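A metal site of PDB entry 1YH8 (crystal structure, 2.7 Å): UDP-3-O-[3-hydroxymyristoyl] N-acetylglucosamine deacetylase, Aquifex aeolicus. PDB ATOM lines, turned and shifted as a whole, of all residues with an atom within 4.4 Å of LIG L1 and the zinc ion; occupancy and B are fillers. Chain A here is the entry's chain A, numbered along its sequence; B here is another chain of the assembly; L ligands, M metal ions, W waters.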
ATOM      1  N   ILE A  17      -5.492 -30.349 -36.569  1.00  0.00           N
ATOM      2  CA  ILE A  17      -5.478 -29.912 -35.190  1.00  0.00           C
ATOM      3  C   ILE A  17      -5.702 -31.056 -34.199  1.00  0.00           C
ATOM      4  O   ILE A  17      -5.145 -31.033 -33.104  1.00  0.00           O
ATOM      5  CB  ILE A  17      -6.534 -28.799 -34.956  1.00  0.00           C
ATOM      6  CG1 ILE A  17      -6.273 -28.142 -33.599  1.00  0.00           C
ATOM      7  CG2 ILE A  17      -7.942 -29.383 -35.018  1.00  0.00           C
ATOM      8  CD1 ILE A  17      -7.266 -27.062 -33.240  1.00  0.00           C
ATOM      9  N   HIS A  18      -6.497 -32.044 -34.586  1.00  0.00           N
ATOM     10  CA  HIS A  18      -6.768 -33.169 -33.688  1.00  0.00           C
ATOM     11  C   HIS A  18      -5.859 -34.381 -33.858  1.00  0.00           C
ATOM     12  O   HIS A  18      -5.345 -34.911 -32.873  1.00  0.00           O
ATOM     13  CB  HIS A  18      -8.223 -33.626 -33.838  1.00  0.00           C
ATOM     14  CG  HIS A  18      -9.212 -32.671 -33.237  1.00  0.00           C
ATOM     15  ND1 HIS A  18      -9.158 -32.278 -31.913  1.00  0.00           N
ATOM     16  CD2 HIS A  18     -10.292 -32.045 -33.767  1.00  0.00           C
ATOM     17  CE1 HIS A  18     -10.154 -31.457 -31.664  1.00  0.00           C
ATOM     18  NE2 HIS A  18     -10.858 -31.292 -32.770  1.00  0.00           N
ATOM     19  N   HIS A  57     -15.837 -31.415 -30.283  1.00  0.00           N
ATOM     20  CA  HIS A  57     -14.578 -30.744 -30.608  1.00  0.00           C
ATOM     21  C   HIS A  57     -14.316 -30.609 -32.105  1.00  0.00           C
ATOM     22  O   HIS A  57     -13.281 -30.062 -32.509  1.00  0.00           O
ATOM     23  CB  HIS A  57     -13.423 -31.473 -29.919  1.00  0.00           C
ATOM     24  CG  HIS A  57     -13.686 -31.747 -28.469  1.00  0.00           C
ATOM     25  ND1 HIS A  57     -13.838 -30.734 -27.545  1.00  0.00           N
ATOM     26  CD2 HIS A  57     -13.921 -32.903 -27.813  1.00  0.00           C
ATOM     27  CE1 HIS A  57     -14.160 -31.260 -26.376  1.00  0.00           C
ATOM     28  NE2 HIS A  57     -14.220 -32.578 -26.515  1.00  0.00           N
ATOM     29  N   GLU A  72     -15.818 -28.438 -40.774  1.00  0.00           N
ATOM     30  CA  GLU A  72     -16.496 -27.155 -40.539  1.00  0.00           C
ATOM     31  C   GLU A  72     -15.878 -25.888 -41.121  1.00  0.00           C
ATOM     32  O   GLU A  72     -16.597 -25.031 -41.632  1.00  0.00           O
ATOM     33  CB  GLU A  72     -16.712 -26.939 -39.046  1.00  0.00           C
ATOM     34  CG  GLU A  72     -15.421 -26.950 -38.213  1.00  0.00           C
ATOM     35  CD  GLU A  72     -15.164 -28.298 -37.555  1.00  0.00           C
ATOM     36  OE1 GLU A  72     -15.437 -29.346 -38.192  1.00  0.00           O
ATOM     37  OE2 GLU A  72     -14.692 -28.304 -36.403  1.00  0.00           O
ATOM     38  N   HIS A  73     -14.564 -25.742 -41.050  1.00  0.00           N
ATOM     39  CA  HIS A  73     -13.928 -24.535 -41.554  1.00  0.00           C
ATOM     40  C   HIS A  73     -13.902 -24.417 -43.072  1.00  0.00           C
ATOM     41  O   HIS A  73     -14.166 -23.344 -43.613  1.00  0.00           O
ATOM     42  CB  HIS A  73     -12.511 -24.411 -40.981  1.00  0.00           C
ATOM     43  CG  HIS A  73     -12.479 -24.230 -39.488  1.00  0.00           C
ATOM     44  ND1 HIS A  73     -11.307 -24.195 -38.769  1.00  0.00           N
ATOM     45  CD2 HIS A  73     -13.475 -24.121 -38.582  1.00  0.00           C
ATOM     46  CE1 HIS A  73     -11.578 -24.068 -37.490  1.00  0.00           C
ATOM     47  NE2 HIS A  73     -12.888 -24.018 -37.347  1.00  0.00           N
ATOM     48  N   THR A 178      -9.578 -20.378 -34.178  1.00  0.00           N
ATOM     49  CA  THR A 178     -10.076 -21.403 -33.259  1.00  0.00           C
ATOM     50  C   THR A 178      -9.588 -21.069 -31.853  1.00  0.00           C
ATOM     51  O   THR A 178      -8.457 -20.592 -31.665  1.00  0.00           O
ATOM     52  CB  THR A 178      -9.526 -22.776 -33.638  1.00  0.00           C
ATOM     53  OG1 THR A 178     -10.034 -23.141 -34.918  1.00  0.00           O
ATOM     54  CG2 THR A 178      -9.913 -23.806 -32.613  1.00  0.00           C
ATOM     55  N   ILE A 185      -8.035 -28.087 -22.193  1.00  0.00           N
ATOM     56  CA  ILE A 185      -6.945 -28.766 -22.855  1.00  0.00           C
ATOM     57  C   ILE A 185      -6.581 -30.137 -22.326  1.00  0.00           C
ATOM     58  O   ILE A 185      -6.246 -31.037 -23.089  1.00  0.00           O
ATOM     59  CB  ILE A 185      -5.682 -27.900 -22.870  1.00  0.00           C
ATOM     60  CG1 ILE A 185      -5.957 -26.593 -23.626  1.00  0.00           C
ATOM     61  CG2 ILE A 185      -4.548 -28.637 -23.562  1.00  0.00           C
ATOM     62  CD1 ILE A 185      -4.751 -25.693 -23.742  1.00  0.00           C
ATOM     63  N   ILE A 188      -9.197 -32.639 -23.833  1.00  0.00           N
ATOM     64  CA  ILE A 188      -8.970 -32.859 -25.257  1.00  0.00           C
ATOM     65  C   ILE A 188      -7.833 -33.851 -25.476  1.00  0.00           C
ATOM     66  O   ILE A 188      -7.962 -34.790 -26.246  1.00  0.00           O
ATOM     67  CB  ILE A 188      -8.595 -31.547 -25.988  1.00  0.00           C
ATOM     68  CG1 ILE A 188      -9.636 -30.467 -25.701  1.00  0.00           C
ATOM     69  CG2 ILE A 188      -8.472 -31.810 -27.488  1.00  0.00           C
ATOM     70  CD1 ILE A 188     -11.012 -30.847 -26.099  1.00  0.00           C
ATOM     71  N   GLY A 194      -6.850 -33.119 -30.151  1.00  0.00           N
ATOM     72  CA  GLY A 194      -5.996 -31.948 -30.076  1.00  0.00           C
ATOM     73  C   GLY A 194      -4.518 -32.194 -30.207  1.00  0.00           C
ATOM     74  O   GLY A 194      -3.709 -31.412 -29.704  1.00  0.00           O
ATOM     75  N   GLY A 197      -2.692 -29.345 -31.932  1.00  0.00           N
ATOM     76  CA  GLY A 197      -2.911 -28.013 -31.394  1.00  0.00           C
ATOM     77  C   GLY A 197      -1.681 -27.300 -30.877  1.00  0.00           C
ATOM     78  O   GLY A 197      -0.783 -27.901 -30.299  1.00  0.00           O
ATOM     79  N   SER A 198      -1.640 -25.988 -31.109  1.00  0.00           N
ATOM     80  CA  SER A 198      -0.545 -25.150 -30.646  1.00  0.00           C
ATOM     81  C   SER A 198      -1.025 -23.709 -30.657  1.00  0.00           C
ATOM     82  O   SER A 198      -2.110 -23.416 -31.149  1.00  0.00           O
ATOM     83  CB  SER A 198       0.659 -25.292 -31.568  1.00  0.00           C
ATOM     84  OG  SER A 198       0.487 -24.509 -32.737  1.00  0.00           O
ATOM     85  N   THR A 202      -4.305 -22.092 -32.424  1.00  0.00           N
ATOM     86  CA  THR A 202      -5.347 -22.019 -31.423  1.00  0.00           C
ATOM     87  C   THR A 202      -5.124 -20.861 -30.453  1.00  0.00           C
ATOM     88  O   THR A 202      -3.988 -20.616 -30.031  1.00  0.00           O
ATOM     89  CB  THR A 202      -5.414 -23.306 -30.560  1.00  0.00           C
ATOM     90  OG1 THR A 202      -5.537 -24.466 -31.396  1.00  0.00           O
ATOM     91  CG2 THR A 202      -6.605 -23.249 -29.612  1.00  0.00           C
ATOM     92  N   VAL A 204      -5.502 -19.802 -26.967  1.00  0.00           N
ATOM     93  CA  VAL A 204      -5.721 -20.393 -25.666  1.00  0.00           C
ATOM     94  C   VAL A 204      -6.060 -19.284 -24.704  1.00  0.00           C
ATOM     95  O   VAL A 204      -5.262 -18.368 -24.500  1.00  0.00           O
ATOM     96  CB  VAL A 204      -4.472 -21.135 -25.187  1.00  0.00           C
ATOM     97  CG1 VAL A 204      -4.757 -21.802 -23.848  1.00  0.00           C
ATOM     98  CG2 VAL A 204      -4.050 -22.160 -26.225  1.00  0.00           C
ATOM     99  N   HIS A 225     -15.736 -16.608 -34.279  1.00  0.00           N
ATOM    100  CA  HIS A 225     -15.361 -17.918 -34.763  1.00  0.00           C
ATOM    101  C   HIS A 225     -16.530 -18.862 -34.596  1.00  0.00           C
ATOM    102  O   HIS A 225     -16.734 -19.741 -35.433  1.00  0.00           O
ATOM    103  CB  HIS A 225     -14.151 -18.483 -33.999  1.00  0.00           C
ATOM    104  CG  HIS A 225     -13.673 -19.783 -34.553  1.00  0.00           C
ATOM    105  ND1 HIS A 225     -12.895 -19.850 -35.695  1.00  0.00           N
ATOM    106  CD2 HIS A 225     -13.958 -21.065 -34.211  1.00  0.00           C
ATOM    107  CE1 HIS A 225     -12.729 -21.118 -36.036  1.00  0.00           C
ATOM    108  NE2 HIS A 225     -13.360 -21.873 -35.146  1.00  0.00           N
ATOM    109  N   ASP A 229     -18.081 -21.278 -37.405  1.00  0.00           N
ATOM    110  CA  ASP A 229     -18.384 -22.696 -37.268  1.00  0.00           C
ATOM    111  C   ASP A 229     -19.837 -23.007 -37.648  1.00  0.00           C
ATOM    112  O   ASP A 229     -20.101 -23.879 -38.487  1.00  0.00           O
ATOM    113  CB  ASP A 229     -18.127 -23.175 -35.836  1.00  0.00           C
ATOM    114  CG  ASP A 229     -16.643 -23.373 -35.531  1.00  0.00           C
ATOM    115  OD1 ASP A 229     -15.875 -23.714 -36.450  1.00  0.00           O
ATOM    116  OD2 ASP A 229     -16.256 -23.229 -34.343  1.00  0.00           O
ATOM    117  N   HIS A 252     -21.032 -27.598 -32.148  1.00  0.00           N
ATOM    118  CA  HIS A 252     -21.240 -28.533 -33.248  1.00  0.00           C
ATOM    119  C   HIS A 252     -22.408 -29.497 -33.067  1.00  0.00           C
ATOM    120  O   HIS A 252     -23.173 -29.718 -33.999  1.00  0.00           O
ATOM    121  CB  HIS A 252     -19.948 -29.298 -33.523  1.00  0.00           C
ATOM    122  CG  HIS A 252     -18.834 -28.421 -33.981  1.00  0.00           C
ATOM    123  ND1 HIS A 252     -18.954 -27.581 -35.074  1.00  0.00           N
ATOM    124  CD2 HIS A 252     -17.597 -28.210 -33.475  1.00  0.00           C
ATOM    125  CE1 HIS A 252     -17.838 -26.894 -35.218  1.00  0.00           C
ATOM    126  NE2 HIS A 252     -16.995 -27.250 -34.261  1.00  0.00           N
ATOM    127  N   ILE B 185       3.616 -19.128 -18.901  1.00  0.00           N
ATOM    128  CA  ILE B 185       3.724 -19.156 -20.349  1.00  0.00           C
ATOM    129  C   ILE B 185       3.461 -17.847 -21.059  1.00  0.00           C
ATOM    130  O   ILE B 185       4.130 -17.541 -22.051  1.00  0.00           O
ATOM    131  CB  ILE B 185       2.809 -20.240 -20.941  1.00  0.00           C
ATOM    132  CG1 ILE B 185       3.244 -21.613 -20.418  1.00  0.00           C
ATOM    133  CG2 ILE B 185       2.935 -20.240 -22.450  1.00  0.00           C
ATOM    134  CD1 ILE B 185       2.418 -22.762 -20.979  1.00  0.00           C
ATOM    135  N   VAL B 204       3.859 -29.015 -18.871  1.00  0.00           N
ATOM    136  CA  VAL B 204       3.106 -27.853 -18.466  1.00  0.00           C
ATOM    137  C   VAL B 204       2.237 -28.250 -17.290  1.00  0.00           C
ATOM    138  O   VAL B 204       1.420 -29.163 -17.383  1.00  0.00           O
ATOM    139  CB  VAL B 204       2.225 -27.335 -19.607  1.00  0.00           C
ATOM    140  CG1 VAL B 204       1.478 -26.084 -19.157  1.00  0.00           C
ATOM    141  CG2 VAL B 204       3.090 -27.041 -20.836  1.00  0.00           C
ATOM    142  N   TYR B 211      -1.065 -30.860 -17.835  1.00  0.00           N
ATOM    143  CA  TYR B 211      -1.595 -30.787 -19.199  1.00  0.00           C
ATOM    144  C   TYR B 211      -1.133 -31.953 -20.077  1.00  0.00           C
ATOM    145  O   TYR B 211      -1.931 -32.540 -20.804  1.00  0.00           O
ATOM    146  CB  TYR B 211      -1.190 -29.466 -19.867  1.00  0.00           C
ATOM    147  CG  TYR B 211      -1.912 -28.240 -19.330  1.00  0.00           C
ATOM    148  CD1 TYR B 211      -1.547 -27.677 -18.105  1.00  0.00           C
ATOM    149  CD2 TYR B 211      -2.967 -27.667 -20.038  1.00  0.00           C
ATOM    150  CE1 TYR B 211      -2.222 -26.572 -17.600  1.00  0.00           C
ATOM    151  CE2 TYR B 211      -3.644 -26.556 -19.545  1.00  0.00           C
ATOM    152  CZ  TYR B 211      -3.265 -26.009 -18.323  1.00  0.00           C
ATOM    153  OH  TYR B 211      -3.944 -24.918 -17.807  1.00  0.00           O
HETATM  154  C1  LIG L   1     -13.229 -25.786 -34.057  1.00  0.00           C
HETATM  155  O1  LIG L   1     -14.345 -25.905 -34.660  1.00  0.00           O
HETATM  156  O2  LIG L   1     -12.555 -24.679 -34.062  1.00  0.00           O
HETATM  157  C2  LIG L   1     -12.691 -27.066 -33.304  1.00  0.00           C
HETATM  158  C3  LIG L   1     -11.326 -26.925 -32.591  1.00  0.00           C
HETATM  159  C4  LIG L   1     -11.342 -26.941 -31.038  1.00  0.00           C
HETATM  160  C5  LIG L   1     -10.307 -27.930 -30.469  1.00  0.00           C
HETATM  161  C6  LIG L   1      -8.930 -27.319 -30.121  1.00  0.00           C
HETATM  162  C7  LIG L   1      -7.969 -28.372 -29.572  1.00  0.00           C
HETATM  163  C8  LIG L   1      -7.059 -27.819 -28.487  1.00  0.00           C
HETATM  164  C9  LIG L   1      -5.679 -27.353 -28.957  1.00  0.00           C
HETATM  165  C10 LIG L   1      -4.645 -27.405 -27.838  1.00  0.00           C
HETATM  166  C11 LIG L   1      -3.611 -26.303 -27.914  1.00  0.00           C
HETATM  167  C12 LIG L   1      -2.456 -26.567 -26.960  1.00  0.00           C
HETATM  168  C13 LIG L   1      -1.838 -25.282 -26.418  1.00  0.00           C
HETATM  169  C14 LIG L   1      -1.212 -25.402 -24.959  1.00  0.00           C
HETATM  170  C15 LIG L   1      -0.588 -25.040 -23.645  1.00  0.00           C
HETATM  171  C16 LIG L   1      -1.069 -24.668 -22.377  1.00  0.00           C
HETATM  172  C1  LG2 L   2      15.500 -25.260 -18.323  1.00  0.00           C
HETATM  173  O1  LG2 L   2      16.634 -25.118 -17.760  1.00  0.00           O
HETATM  174  O2  LG2 L   2      14.875 -26.391 -18.371  1.00  0.00           O
HETATM  175  C2  LG2 L   2      14.880 -23.976 -18.978  1.00  0.00           C
HETATM  176  C3  LG2 L   2      13.515 -24.173 -19.663  1.00  0.00           C
HETATM  177  C4  LG2 L   2      12.341 -23.369 -19.090  1.00  0.00           C
HETATM  178  C5  LG2 L   2      11.576 -22.626 -20.184  1.00  0.00           C
HETATM  179  C6  LG2 L   2      10.379 -23.381 -20.738  1.00  0.00           C
HETATM  180  C7  LG2 L   2       9.679 -22.593 -21.813  1.00  0.00           C
HETATM  181  C8  LG2 L   2       8.177 -22.799 -21.742  1.00  0.00           C
HETATM  182  C9  LG2 L   2       7.464 -22.767 -23.094  1.00  0.00           C
HETATM  183  C10 LG2 L   2       5.954 -22.914 -22.926  1.00  0.00           C
HETATM  184  C11 LG2 L   2       5.417 -24.247 -23.411  1.00  0.00           C
HETATM  185  C12 LG2 L   2       4.422 -24.022 -24.536  1.00  0.00           C
HETATM  186  C13 LG2 L   2       3.473 -25.205 -24.721  1.00  0.00           C
HETATM  187  C14 LG2 L   2       2.442 -25.016 -25.898  1.00  0.00           C
HETATM  188  C15 LG2 L   2       1.869 -24.824 -27.282  1.00  0.00           C
HETATM  189  C16 LG2 L   2       2.270 -24.143 -28.441  1.00  0.00           C
HETATM  190 ZN    ZN M   1     -13.955 -23.743 -35.640  1.00  0.00          ZN
HETATM  191  O   HOH W   1     -13.355 -27.913 -28.797  1.00  0.00           O
HETATM  192  O   HOH W   2     -12.740 -23.092 -31.106  1.00  0.00           O
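A ring nitrogen (NE2) of His 252 lies close to an oxygen (O1) of LIG L1.
The side-chain hydroxyl (OG1) of Thr 178 lies close to an oxygen (O2) of LIG L1 (3.1 Å).
The side-chain carboxylate (OE2) of Glu 72 sits at hydrogen-bond distance from a ring nitrogen (NE2) of His 252 (3.3 Å).
The backbone carbonyl oxygen (O) of His 57 lies within hydrogen-bond range of a ring nitrogen (NE2) of His 18, at 2.7 Å.
O of Ile 17 lies within hydrogen-bond range of N of Gly 197, 3.2 Å away.
ND1 of His 18 is in hydrogen-bond range of N of Gly 194, 3.0 Å away.
OE2 of Glu 72 sits close to O1 of LIG L1, 3.0 Å away.
Merely in contact with LIG L1: His 57, Ile 17, Gly 197, His 18, Ile 185 of chain A, Ser 198, Thr 202 and Val 204 of chain A.
Hydrophobic or aromatic side chains that line LIG L1: Ile 17, His 18, His 73, Ile 185 of chain A, Val 204 of chain A, His 225 and His 252.
14 residues have an atom within 4 Å of LIG L1: Ile 17, His 18, His 57, Glu 72, His 73, Thr 178, Ile 185 of chain A, Gly 197, Ser 198, Thr 202, Val 204 of chain A, His 225, Asp 229 and His 252.
Along chain A the residues within 4 Å of LIG L1 span positions 17 to 252.
Within 4 Å of the zinc ion: His 73, His 225 and Asp 229.
The zinc ion is bound by NE2 of His 225 (2.0 Å), NE2 of His 73 (2.0 Å), OD1 of Asp 229 (2.1 Å), O2 of LIG L1 (2.3 Å) and O1 of LIG L1 (2.4 Å).
The zinc ion has five donor atoms within binding distance.
Slightly farther from the zinc ion lies the side-chain carboxylate (OD2) of Asp 229 (2.7 Å).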
